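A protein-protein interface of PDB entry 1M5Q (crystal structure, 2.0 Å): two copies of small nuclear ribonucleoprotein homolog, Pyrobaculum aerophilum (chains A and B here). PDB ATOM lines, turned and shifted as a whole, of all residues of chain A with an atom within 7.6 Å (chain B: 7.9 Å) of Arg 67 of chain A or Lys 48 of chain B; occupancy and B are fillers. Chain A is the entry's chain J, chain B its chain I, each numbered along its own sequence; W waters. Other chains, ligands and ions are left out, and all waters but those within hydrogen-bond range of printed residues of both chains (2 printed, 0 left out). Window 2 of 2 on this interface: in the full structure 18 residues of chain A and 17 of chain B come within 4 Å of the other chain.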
ATOM      1  N   ARG A  11      -3.981  18.465  -2.790  1.00  0.00           N
ATOM      2  CA  ARG A  11      -3.882  17.007  -2.736  1.00  0.00           C
ATOM      3  C   ARG A  11      -5.035  16.463  -1.907  1.00  0.00           C
ATOM      4  O   ARG A  11      -5.604  17.181  -1.073  1.00  0.00           O
ATOM      5  CB  ARG A  11      -2.556  16.584  -2.091  1.00  0.00           C
ATOM      6  CG  ARG A  11      -1.308  17.117  -2.772  1.00  0.00           C
ATOM      7  CD  ARG A  11      -1.173  16.519  -4.187  1.00  0.00           C
ATOM      8  NE  ARG A  11      -0.574  15.174  -4.227  1.00  0.00           N
ATOM      9  CZ  ARG A  11       0.739  14.959  -4.266  1.00  0.00           C
ATOM     10  NH1 ARG A  11       1.561  15.992  -4.265  1.00  0.00           N
ATOM     11  NH2 ARG A  11       1.233  13.721  -4.341  1.00  0.00           N
ATOM     12  N   ASP A  63      -5.162  12.381   7.539  1.00  0.00           N
ATOM     13  CA  ASP A  63      -4.337  11.336   6.914  1.00  0.00           C
ATOM     14  C   ASP A  63      -4.169  11.571   5.439  1.00  0.00           C
ATOM     15  O   ASP A  63      -5.113  11.994   4.760  1.00  0.00           O
ATOM     16  CB  ASP A  63      -4.985   9.970   7.097  1.00  0.00           C
ATOM     17  CG  ASP A  63      -5.656   9.828   8.456  1.00  0.00           C
ATOM     18  OD1 ASP A  63      -4.995  10.232   9.433  1.00  0.00           O
ATOM     19  OD2 ASP A  63      -6.816   9.322   8.548  1.00  0.00           O
ATOM     20  N   SER A  64      -2.962  11.300   4.947  1.00  0.00           N
ATOM     21  CA  SER A  64      -2.673  11.402   3.511  1.00  0.00           C
ATOM     22  C   SER A  64      -3.424  10.198   2.931  1.00  0.00           C
ATOM     23  O   SER A  64      -3.426   9.130   3.530  1.00  0.00           O
ATOM     24  CB  SER A  64      -1.189  11.182   3.277  1.00  0.00           C
ATOM     25  OG  SER A  64      -0.875   9.909   3.869  1.00  0.00           O
ATOM     26  N   THR A  65      -4.042  10.330   1.771  1.00  0.00           N
ATOM     27  CA  THR A  65      -4.787   9.183   1.245  1.00  0.00           C
ATOM     28  C   THR A  65      -4.125   8.564  -0.004  1.00  0.00           C
ATOM     29  O   THR A  65      -4.545   7.515  -0.453  1.00  0.00           O
ATOM     30  CB  THR A  65      -6.253   9.581   0.894  1.00  0.00           C
ATOM     31  OG1 THR A  65      -6.216  10.692   0.000  1.00  0.00           O
ATOM     32  CG2 THR A  65      -7.061   9.980   2.144  1.00  0.00           C
ATOM     33  N   GLU A  66      -3.107   9.202  -0.571  1.00  0.00           N
ATOM     34  CA  GLU A  66      -2.464   8.630  -1.772  1.00  0.00           C
ATOM     35  C   GLU A  66      -1.309   7.708  -1.409  1.00  0.00           C
ATOM     36  O   GLU A  66      -0.587   7.938  -0.443  1.00  0.00           O
ATOM     37  CB  GLU A  66      -1.948   9.738  -2.704  1.00  0.00           C
ATOM     38  CG  GLU A  66      -3.021  10.702  -3.189  1.00  0.00           C
ATOM     39  CD  GLU A  66      -2.439  11.970  -3.820  1.00  0.00           C
ATOM     40  OE1 GLU A  66      -3.198  12.970  -3.995  1.00  0.00           O
ATOM     41  OE2 GLU A  66      -1.227  11.967  -4.146  1.00  0.00           O
ATOM     42  N   ARG A  67      -1.149   6.645  -2.178  1.00  0.00           N
ATOM     43  CA  ARG A  67      -0.059   5.735  -1.954  1.00  0.00           C
ATOM     44  C   ARG A  67       1.148   6.359  -2.629  1.00  0.00           C
ATOM     45  O   ARG A  67       0.994   7.063  -3.603  1.00  0.00           O
ATOM     46  CB  ARG A  67      -0.343   4.372  -2.595  1.00  0.00           C
ATOM     47  CG  ARG A  67      -0.599   3.220  -1.585  1.00  0.00           C
ATOM     48  CD  ARG A  67      -0.523   1.820  -2.253  1.00  0.00           C
ATOM     49  NE  ARG A  67       0.709   1.087  -1.902  1.00  0.00           N
ATOM     50  CZ  ARG A  67       0.987   0.589  -0.688  1.00  0.00           C
ATOM     51  NH1 ARG A  67       0.114   0.723   0.319  1.00  0.00           N
ATOM     52  NH2 ARG A  67       2.154  -0.019  -0.466  1.00  0.00           N
ATOM     53  N   ARG A  68       2.339   6.158  -2.075  1.00  0.00           N
ATOM     54  CA  ARG A  68       3.564   6.650  -2.703  1.00  0.00           C
ATOM     55  C   ARG A  68       3.733   5.891  -4.050  1.00  0.00           C
ATOM     56  O   ARG A  68       3.162   4.822  -4.261  1.00  0.00           O
ATOM     57  CB  ARG A  68       4.785   6.354  -1.829  1.00  0.00           C
ATOM     58  CG  ARG A  68       4.927   7.229  -0.574  1.00  0.00           C
ATOM     59  CD  ARG A  68       5.021   8.733  -0.917  1.00  0.00           C
ATOM     60  NE  ARG A  68       5.308   9.522   0.290  1.00  0.00           N
ATOM     61  CZ  ARG A  68       5.377  10.849   0.323  1.00  0.00           C
ATOM     62  NH1 ARG A  68       5.172  11.540  -0.807  1.00  0.00           N
ATOM     63  NH2 ARG A  68       5.663  11.472   1.470  1.00  0.00           N
ATOM     64  N   ILE A  69       4.511   6.458  -4.956  1.00  0.00           N
ATOM     65  CA  ILE A  69       4.762   5.822  -6.252  1.00  0.00           C
ATOM     66  C   ILE A  69       5.533   4.506  -6.088  1.00  0.00           C
ATOM     67  O   ILE A  69       6.430   4.388  -5.236  1.00  0.00           O
ATOM     68  CB  ILE A  69       5.573   6.792  -7.161  1.00  0.00           C
ATOM     69  CG1 ILE A  69       4.638   7.856  -7.694  1.00  0.00           C
ATOM     70  CG2 ILE A  69       6.282   6.054  -8.299  1.00  0.00           C
ATOM     71  CD1 ILE A  69       5.389   9.030  -8.257  1.00  0.00           C
ATOM     72  N   ASP A  70       5.164   3.514  -6.889  1.00  0.00           N
ATOM     73  CA  ASP A  70       5.851   2.222  -6.899  1.00  0.00           C
ATOM     74  C   ASP A  70       7.165   2.434  -7.664  1.00  0.00           C
ATOM     75  O   ASP A  70       7.169   2.623  -8.884  1.00  0.00           O
ATOM     76  CB  ASP A  70       5.002   1.179  -7.619  1.00  0.00           C
ATOM     77  CG  ASP A  70       5.746  -0.123  -7.821  1.00  0.00           C
ATOM     78  OD1 ASP A  70       5.094  -1.123  -8.158  1.00  0.00           O
ATOM     79  OD2 ASP A  70       6.987  -0.140  -7.646  1.00  0.00           O
ATOM     80  N   GLU A 105      10.884   8.002  -3.410  1.00  0.00           N
ATOM     81  CA  GLU A 105       9.437   8.134  -3.457  1.00  0.00           C
ATOM     82  C   GLU A 105       8.963   9.540  -3.129  1.00  0.00           C
ATOM     83  O   GLU A 105       7.781   9.805  -3.231  1.00  0.00           O
ATOM     84  CB  GLU A 105       8.728   7.106  -2.543  1.00  0.00           C
ATOM     85  CG  GLU A 105       9.177   7.072  -1.089  1.00  0.00           C
ATOM     86  CD  GLU A 105       8.360   6.089  -0.217  1.00  0.00           C
ATOM     87  OE1 GLU A 105       7.800   5.114  -0.766  1.00  0.00           O
ATOM     88  OE2 GLU A 105       8.312   6.283   1.031  1.00  0.00           O
ATOM     89  N   PHE A 125       2.948   9.758 -12.716  1.00  0.00           N
ATOM     90  CA  PHE A 125       2.574   8.652 -11.831  1.00  0.00           C
ATOM     91  C   PHE A 125       1.591   9.215 -10.797  1.00  0.00           C
ATOM     92  O   PHE A 125       0.581   8.595 -10.448  1.00  0.00           O
ATOM     93  CB  PHE A 125       3.791   8.091 -11.093  1.00  0.00           C
ATOM     94  CG  PHE A 125       4.469   6.945 -11.803  1.00  0.00           C
ATOM     95  CD1 PHE A 125       5.269   7.172 -12.905  1.00  0.00           C
ATOM     96  CD2 PHE A 125       4.301   5.634 -11.359  1.00  0.00           C
ATOM     97  CE1 PHE A 125       5.894   6.107 -13.559  1.00  0.00           C
ATOM     98  CE2 PHE A 125       4.924   4.554 -12.006  1.00  0.00           C
ATOM     99  CZ  PHE A 125       5.722   4.792 -13.108  1.00  0.00           C
ATOM    100  N   LEU A 126       1.909  10.410 -10.309  1.00  0.00           N
ATOM    101  CA  LEU A 126       1.071  11.057  -9.317  1.00  0.00           C
ATOM    102  C   LEU A 126      -0.263  11.510  -9.899  1.00  0.00           C
ATOM    103  O   LEU A 126      -1.233  11.571  -9.154  1.00  0.00           O
ATOM    104  CB  LEU A 126       1.794  12.261  -8.682  1.00  0.00           C
ATOM    105  CG  LEU A 126       3.072  12.042  -7.854  1.00  0.00           C
ATOM    106  CD1 LEU A 126       3.697  13.428  -7.591  1.00  0.00           C
ATOM    107  CD2 LEU A 126       2.774  11.256  -6.533  1.00  0.00           C
ATOM    108  N   TYR B  23      -3.256   4.042  16.514  1.00  0.00           N
ATOM    109  CA  TYR B  23      -2.382   4.015  15.334  1.00  0.00           C
ATOM    110  C   TYR B  23      -0.955   3.522  15.665  1.00  0.00           C
ATOM    111  O   TYR B  23      -0.359   3.888  16.692  1.00  0.00           O
ATOM    112  CB  TYR B  23      -2.289   5.406  14.673  1.00  0.00           C
ATOM    113  CG  TYR B  23      -3.489   5.738  13.869  1.00  0.00           C
ATOM    114  CD1 TYR B  23      -3.526   5.464  12.484  1.00  0.00           C
ATOM    115  CD2 TYR B  23      -4.660   6.172  14.493  1.00  0.00           C
ATOM    116  CE1 TYR B  23      -4.734   5.601  11.737  1.00  0.00           C
ATOM    117  CE2 TYR B  23      -5.879   6.313  13.759  1.00  0.00           C
ATOM    118  CZ  TYR B  23      -5.908   6.017  12.398  1.00  0.00           C
ATOM    119  OH  TYR B  23      -7.117   6.053  11.734  1.00  0.00           O
ATOM    120  N   LYS B  24      -0.422   2.656  14.811  1.00  0.00           N
ATOM    121  CA  LYS B  24       0.936   2.153  15.014  1.00  0.00           C
ATOM    122  C   LYS B  24       1.751   2.526  13.769  1.00  0.00           C
ATOM    123  O   LYS B  24       1.303   2.337  12.619  1.00  0.00           O
ATOM    124  CB  LYS B  24       0.859   0.643  15.233  1.00  0.00           C
ATOM    125  CG  LYS B  24       2.147  -0.129  15.085  1.00  0.00           C
ATOM    126  CD  LYS B  24       2.065  -1.498  15.855  1.00  0.00           C
ATOM    127  CE  LYS B  24       2.213  -1.268  17.401  1.00  0.00           C
ATOM    128  NZ  LYS B  24       1.846  -2.396  18.336  1.00  0.00           N
ATOM    129  N   ASN B  40       3.672   5.735   7.532  1.00  0.00           N
ATOM    130  CA  ASN B  40       3.257   4.360   7.256  1.00  0.00           C
ATOM    131  C   ASN B  40       2.622   3.722   8.493  1.00  0.00           C
ATOM    132  O   ASN B  40       3.058   2.677   8.998  1.00  0.00           O
ATOM    133  CB  ASN B  40       4.478   3.530   6.767  1.00  0.00           C
ATOM    134  CG  ASN B  40       4.984   3.994   5.406  1.00  0.00           C
ATOM    135  OD1 ASN B  40       4.207   4.235   4.497  1.00  0.00           O
ATOM    136  ND2 ASN B  40       6.289   4.132   5.273  1.00  0.00           N
ATOM    137  N   ALA B  41       1.600   4.402   9.000  1.00  0.00           N
ATOM    138  CA  ALA B  41       0.900   3.951  10.183  1.00  0.00           C
ATOM    139  C   ALA B  41      -0.356   3.189   9.790  1.00  0.00           C
ATOM    140  O   ALA B  41      -0.899   3.325   8.678  1.00  0.00           O
ATOM    141  CB  ALA B  41       0.521   5.144  11.052  1.00  0.00           C
ATOM    142  N   SER B  42      -0.844   2.431  10.737  1.00  0.00           N
ATOM    143  CA  SER B  42      -2.015   1.643  10.520  1.00  0.00           C
ATOM    144  C   SER B  42      -2.880   1.709  11.789  1.00  0.00           C
ATOM    145  O   SER B  42      -2.357   1.894  12.890  1.00  0.00           O
ATOM    146  CB  SER B  42      -1.574   0.173  10.303  1.00  0.00           C
ATOM    147  OG  SER B  42      -2.657  -0.713  10.527  1.00  0.00           O
ATOM    148  N   ASN B  43      -4.186   1.526  11.646  1.00  0.00           N
ATOM    149  CA  ASN B  43      -5.031   1.452  12.828  1.00  0.00           C
ATOM    150  C   ASN B  43      -5.485   0.005  13.019  1.00  0.00           C
ATOM    151  O   ASN B  43      -5.185  -0.861  12.188  1.00  0.00           O
ATOM    152  CB  ASN B  43      -6.255   2.371  12.732  1.00  0.00           C
ATOM    153  CG  ASN B  43      -7.055   2.153  11.496  1.00  0.00           C
ATOM    154  OD1 ASN B  43      -7.171   1.010  10.984  1.00  0.00           O
ATOM    155  ND2 ASN B  43      -7.650   3.251  10.988  1.00  0.00           N
ATOM    156  N   ALA B  45      -8.208  -1.400  12.507  1.00  0.00           N
ATOM    157  CA  ALA B  45      -9.016  -1.887  11.365  1.00  0.00           C
ATOM    158  C   ALA B  45      -8.170  -2.312  10.159  1.00  0.00           C
ATOM    159  O   ALA B  45      -8.692  -2.789   9.177  1.00  0.00           O
ATOM    160  CB  ALA B  45      -9.994  -0.842  10.923  1.00  0.00           C
ATOM    161  N   GLY B  46      -6.867  -2.136  10.225  1.00  0.00           N
ATOM    162  CA  GLY B  46      -6.032  -2.527   9.098  1.00  0.00           C
ATOM    163  C   GLY B  46      -5.833  -1.479   8.012  1.00  0.00           C
ATOM    164  O   GLY B  46      -5.227  -1.770   6.990  1.00  0.00           O
ATOM    165  N   GLU B  47      -6.347  -0.268   8.218  1.00  0.00           N
ATOM    166  CA  GLU B  47      -6.196   0.807   7.260  1.00  0.00           C
ATOM    167  C   GLU B  47      -4.796   1.387   7.430  1.00  0.00           C
ATOM    168  O   GLU B  47      -4.344   1.567   8.551  1.00  0.00           O
ATOM    169  CB  GLU B  47      -7.237   1.909   7.555  1.00  0.00           C
ATOM    170  CG  GLU B  47      -8.674   1.369   7.636  1.00  0.00           C
ATOM    171  CD  GLU B  47      -9.675   2.455   7.897  1.00  0.00           C
ATOM    172  OE1 GLU B  47      -9.810   2.875   9.050  1.00  0.00           O
ATOM    173  OE2 GLU B  47     -10.319   2.925   6.943  1.00  0.00           O
ATOM    174  N   LYS B  48      -4.094   1.685   6.352  1.00  0.00           N
ATOM    175  CA  LYS B  48      -2.766   2.269   6.531  1.00  0.00           C
ATOM    176  C   LYS B  48      -2.622   3.509   5.640  1.00  0.00           C
ATOM    177  O   LYS B  48      -3.288   3.642   4.619  1.00  0.00           O
ATOM    178  CB  LYS B  48      -1.675   1.223   6.268  1.00  0.00           C
ATOM    179  CG  LYS B  48      -1.707   0.687   4.889  1.00  0.00           C
ATOM    180  CD  LYS B  48      -1.052  -0.716   4.826  1.00  0.00           C
ATOM    181  CE  LYS B  48      -0.857  -1.160   3.352  1.00  0.00           C
ATOM    182  NZ  LYS B  48       0.213  -2.143   3.304  1.00  0.00           N
ATOM    183  N   PHE B  49      -1.765   4.430   6.063  1.00  0.00           N
ATOM    184  CA  PHE B  49      -1.572   5.701   5.384  1.00  0.00           C
ATOM    185  C   PHE B  49      -0.133   6.010   5.444  1.00  0.00           C
ATOM    186  O   PHE B  49       0.501   5.726   6.451  1.00  0.00           O
ATOM    187  CB  PHE B  49      -2.314   6.802   6.147  1.00  0.00           C
ATOM    188  CG  PHE B  49      -3.707   6.434   6.513  1.00  0.00           C
ATOM    189  CD1 PHE B  49      -3.980   5.810   7.724  1.00  0.00           C
ATOM    190  CD2 PHE B  49      -4.737   6.641   5.609  1.00  0.00           C
ATOM    191  CE1 PHE B  49      -5.280   5.387   8.034  1.00  0.00           C
ATOM    192  CE2 PHE B  49      -6.034   6.216   5.908  1.00  0.00           C
ATOM    193  CZ  PHE B  49      -6.297   5.587   7.129  1.00  0.00           C
ATOM    194  N   ASN B  50       0.380   6.613   4.390  1.00  0.00           N
ATOM    195  CA  ASN B  50       1.783   6.951   4.359  1.00  0.00           C
ATOM    196  C   ASN B  50       2.029   8.019   5.438  1.00  0.00           C
ATOM    197  O   ASN B  50       3.112   8.060   6.027  1.00  0.00           O
ATOM    198  CB  ASN B  50       2.195   7.397   2.955  1.00  0.00           C
ATOM    199  CG  ASN B  50       3.522   8.178   2.945  1.00  0.00           C
ATOM    200  OD1 ASN B  50       3.512   9.407   2.948  1.00  0.00           O
ATOM    201  ND2 ASN B  50       4.658   7.472   2.950  1.00  0.00           N
ATOM    202  N   ARG B  51       1.050   8.881   5.713  1.00  0.00           N
ATOM    203  CA  ARG B  51       1.219   9.837   6.821  1.00  0.00           C
ATOM    204  C   ARG B  51      -0.023  10.114   7.635  1.00  0.00           C
ATOM    205  O   ARG B  51      -1.096  10.274   7.104  1.00  0.00           O
ATOM    206  CB  ARG B  51       1.788  11.201   6.366  1.00  0.00           C
ATOM    207  CG  ARG B  51       3.337  11.181   6.253  1.00  0.00           C
ATOM    208  CD  ARG B  51       3.825  12.505   5.754  1.00  0.00           C
ATOM    209  NE  ARG B  51       3.342  12.830   4.411  1.00  0.00           N
ATOM    210  CZ  ARG B  51       3.553  14.002   3.817  1.00  0.00           C
ATOM    211  NH1 ARG B  51       4.213  14.953   4.481  1.00  0.00           N
ATOM    212  NH2 ARG B  51       3.199  14.206   2.543  1.00  0.00           N
ATOM    213  N   VAL B  52       0.138  10.151   8.943  1.00  0.00           N
ATOM    214  CA  VAL B  52      -0.979  10.494   9.785  1.00  0.00           C
ATOM    215  C   VAL B  52      -0.569  11.689  10.703  1.00  0.00           C
ATOM    216  O   VAL B  52       0.405  11.624  11.433  1.00  0.00           O
ATOM    217  CB  VAL B  52      -1.424   9.306  10.621  1.00  0.00           C
ATOM    218  CG1 VAL B  52      -2.520   9.716  11.515  1.00  0.00           C
ATOM    219  CG2 VAL B  52      -1.897   8.175   9.678  1.00  0.00           C
HETATM  220  O   HOH W   1       7.546   8.580   2.712  1.00  0.00           O
HETATM  221  O   HOH W   2      -1.526   6.931   2.090  1.00  0.00           O
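Of the printed residues of chain B, Asp 63 of chain A touches Phe 49 (3.7 Å), Arg 51 (3.4 Å) and Val 52 (3.3 Å).
Of the printed residues of chain B, Ser 64 of chain A touches Phe 49 (3.5 Å), Asn 50 (3.6 Å) and Arg 51 (2.9 Å).
Glu 105 of chain A touches none of the printed residues of chain B.
Leu 126 of chain A touches none of the printed residues of chain B.
Printed residues of chain A within 4 Å of Lys 48 of chain B: Arg 67 (3.7 Å).
Of the printed residues of chain A, Phe 49 of chain B touches Asp 63 (3.7 Å) and Ser 64 (3.5 Å).
Printed residues of chain A within 4 Å of Arg 51 of chain B: Asp 63 (3.4 Å), Ser 64 (2.9 Å) and Arg 68 (3.8 Å).
The nearest residue of chain B that does not touch Arg 67 of chain A is Asn 50 of chain B (5.7 Å).
No position is printed for both chains.
Phe 49 of chain B touches Asp 63 of chain A (CD2 to CB, 3.7 Å).
Asp 63 of chain A touches Arg 51 of chain B.
Val 52 of chain B touches Asp 63 of chain A (CG1 to OD1, 3.3 Å).
CD2 of Phe 49 of chain B touches O of Ser 64 of chain A, at 3.5 Å.
Ser 64 of chain A touches Asn 50 of chain B.
Arg 67 of chain A touches Lys 48 of chain B.
Arg 68 of chain A touches Arg 51 of chain B.
OG of Ser 64 of chain A lies within hydrogen-bond range of N of Arg 51 of chain B (2.9 Å).
NE of Arg 68 of chain A sits at hydrogen-bond distance from OD1 of Asn 50 of chain B, 3.2 Å away.
Of the 14 printed residues of chain B, 5 touch a printed residue of chain A.
Hydrophobic or aromatic side chains of chain B within 4 Å of the printed part of chain A: Phe 49 and Val 52.
Water W2 lies within hydrogen-bond range of O of Glu 66 of chain A (2.9 Å), N of Asn 50 of chain B (3.0 Å) and O of Ser 64 of chain A (3.2 Å).
Water W1 lies within hydrogen-bond range of the side-chain carboxylate of Glu 105 of chain A (2.9 Å), the side-chain amide nitrogen of Asn 50 of chain B (3.1 Å) and the guanidinium group of Arg 68 of chain A (3.4 Å).
O of Ala 41 of chain B is in hydrogen-bond range of N of Phe 49 of chain B (3.0 Å).
N of Asn 40 of chain B sits at hydrogen-bond distance from O of Asn 50 of chain B (2.8 Å).
The backbone NH (N) of Asn 40 of chain B sits close to the backbone carbonyl oxygen (O) of Phe 49 of chain B, 3.4 Å away.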
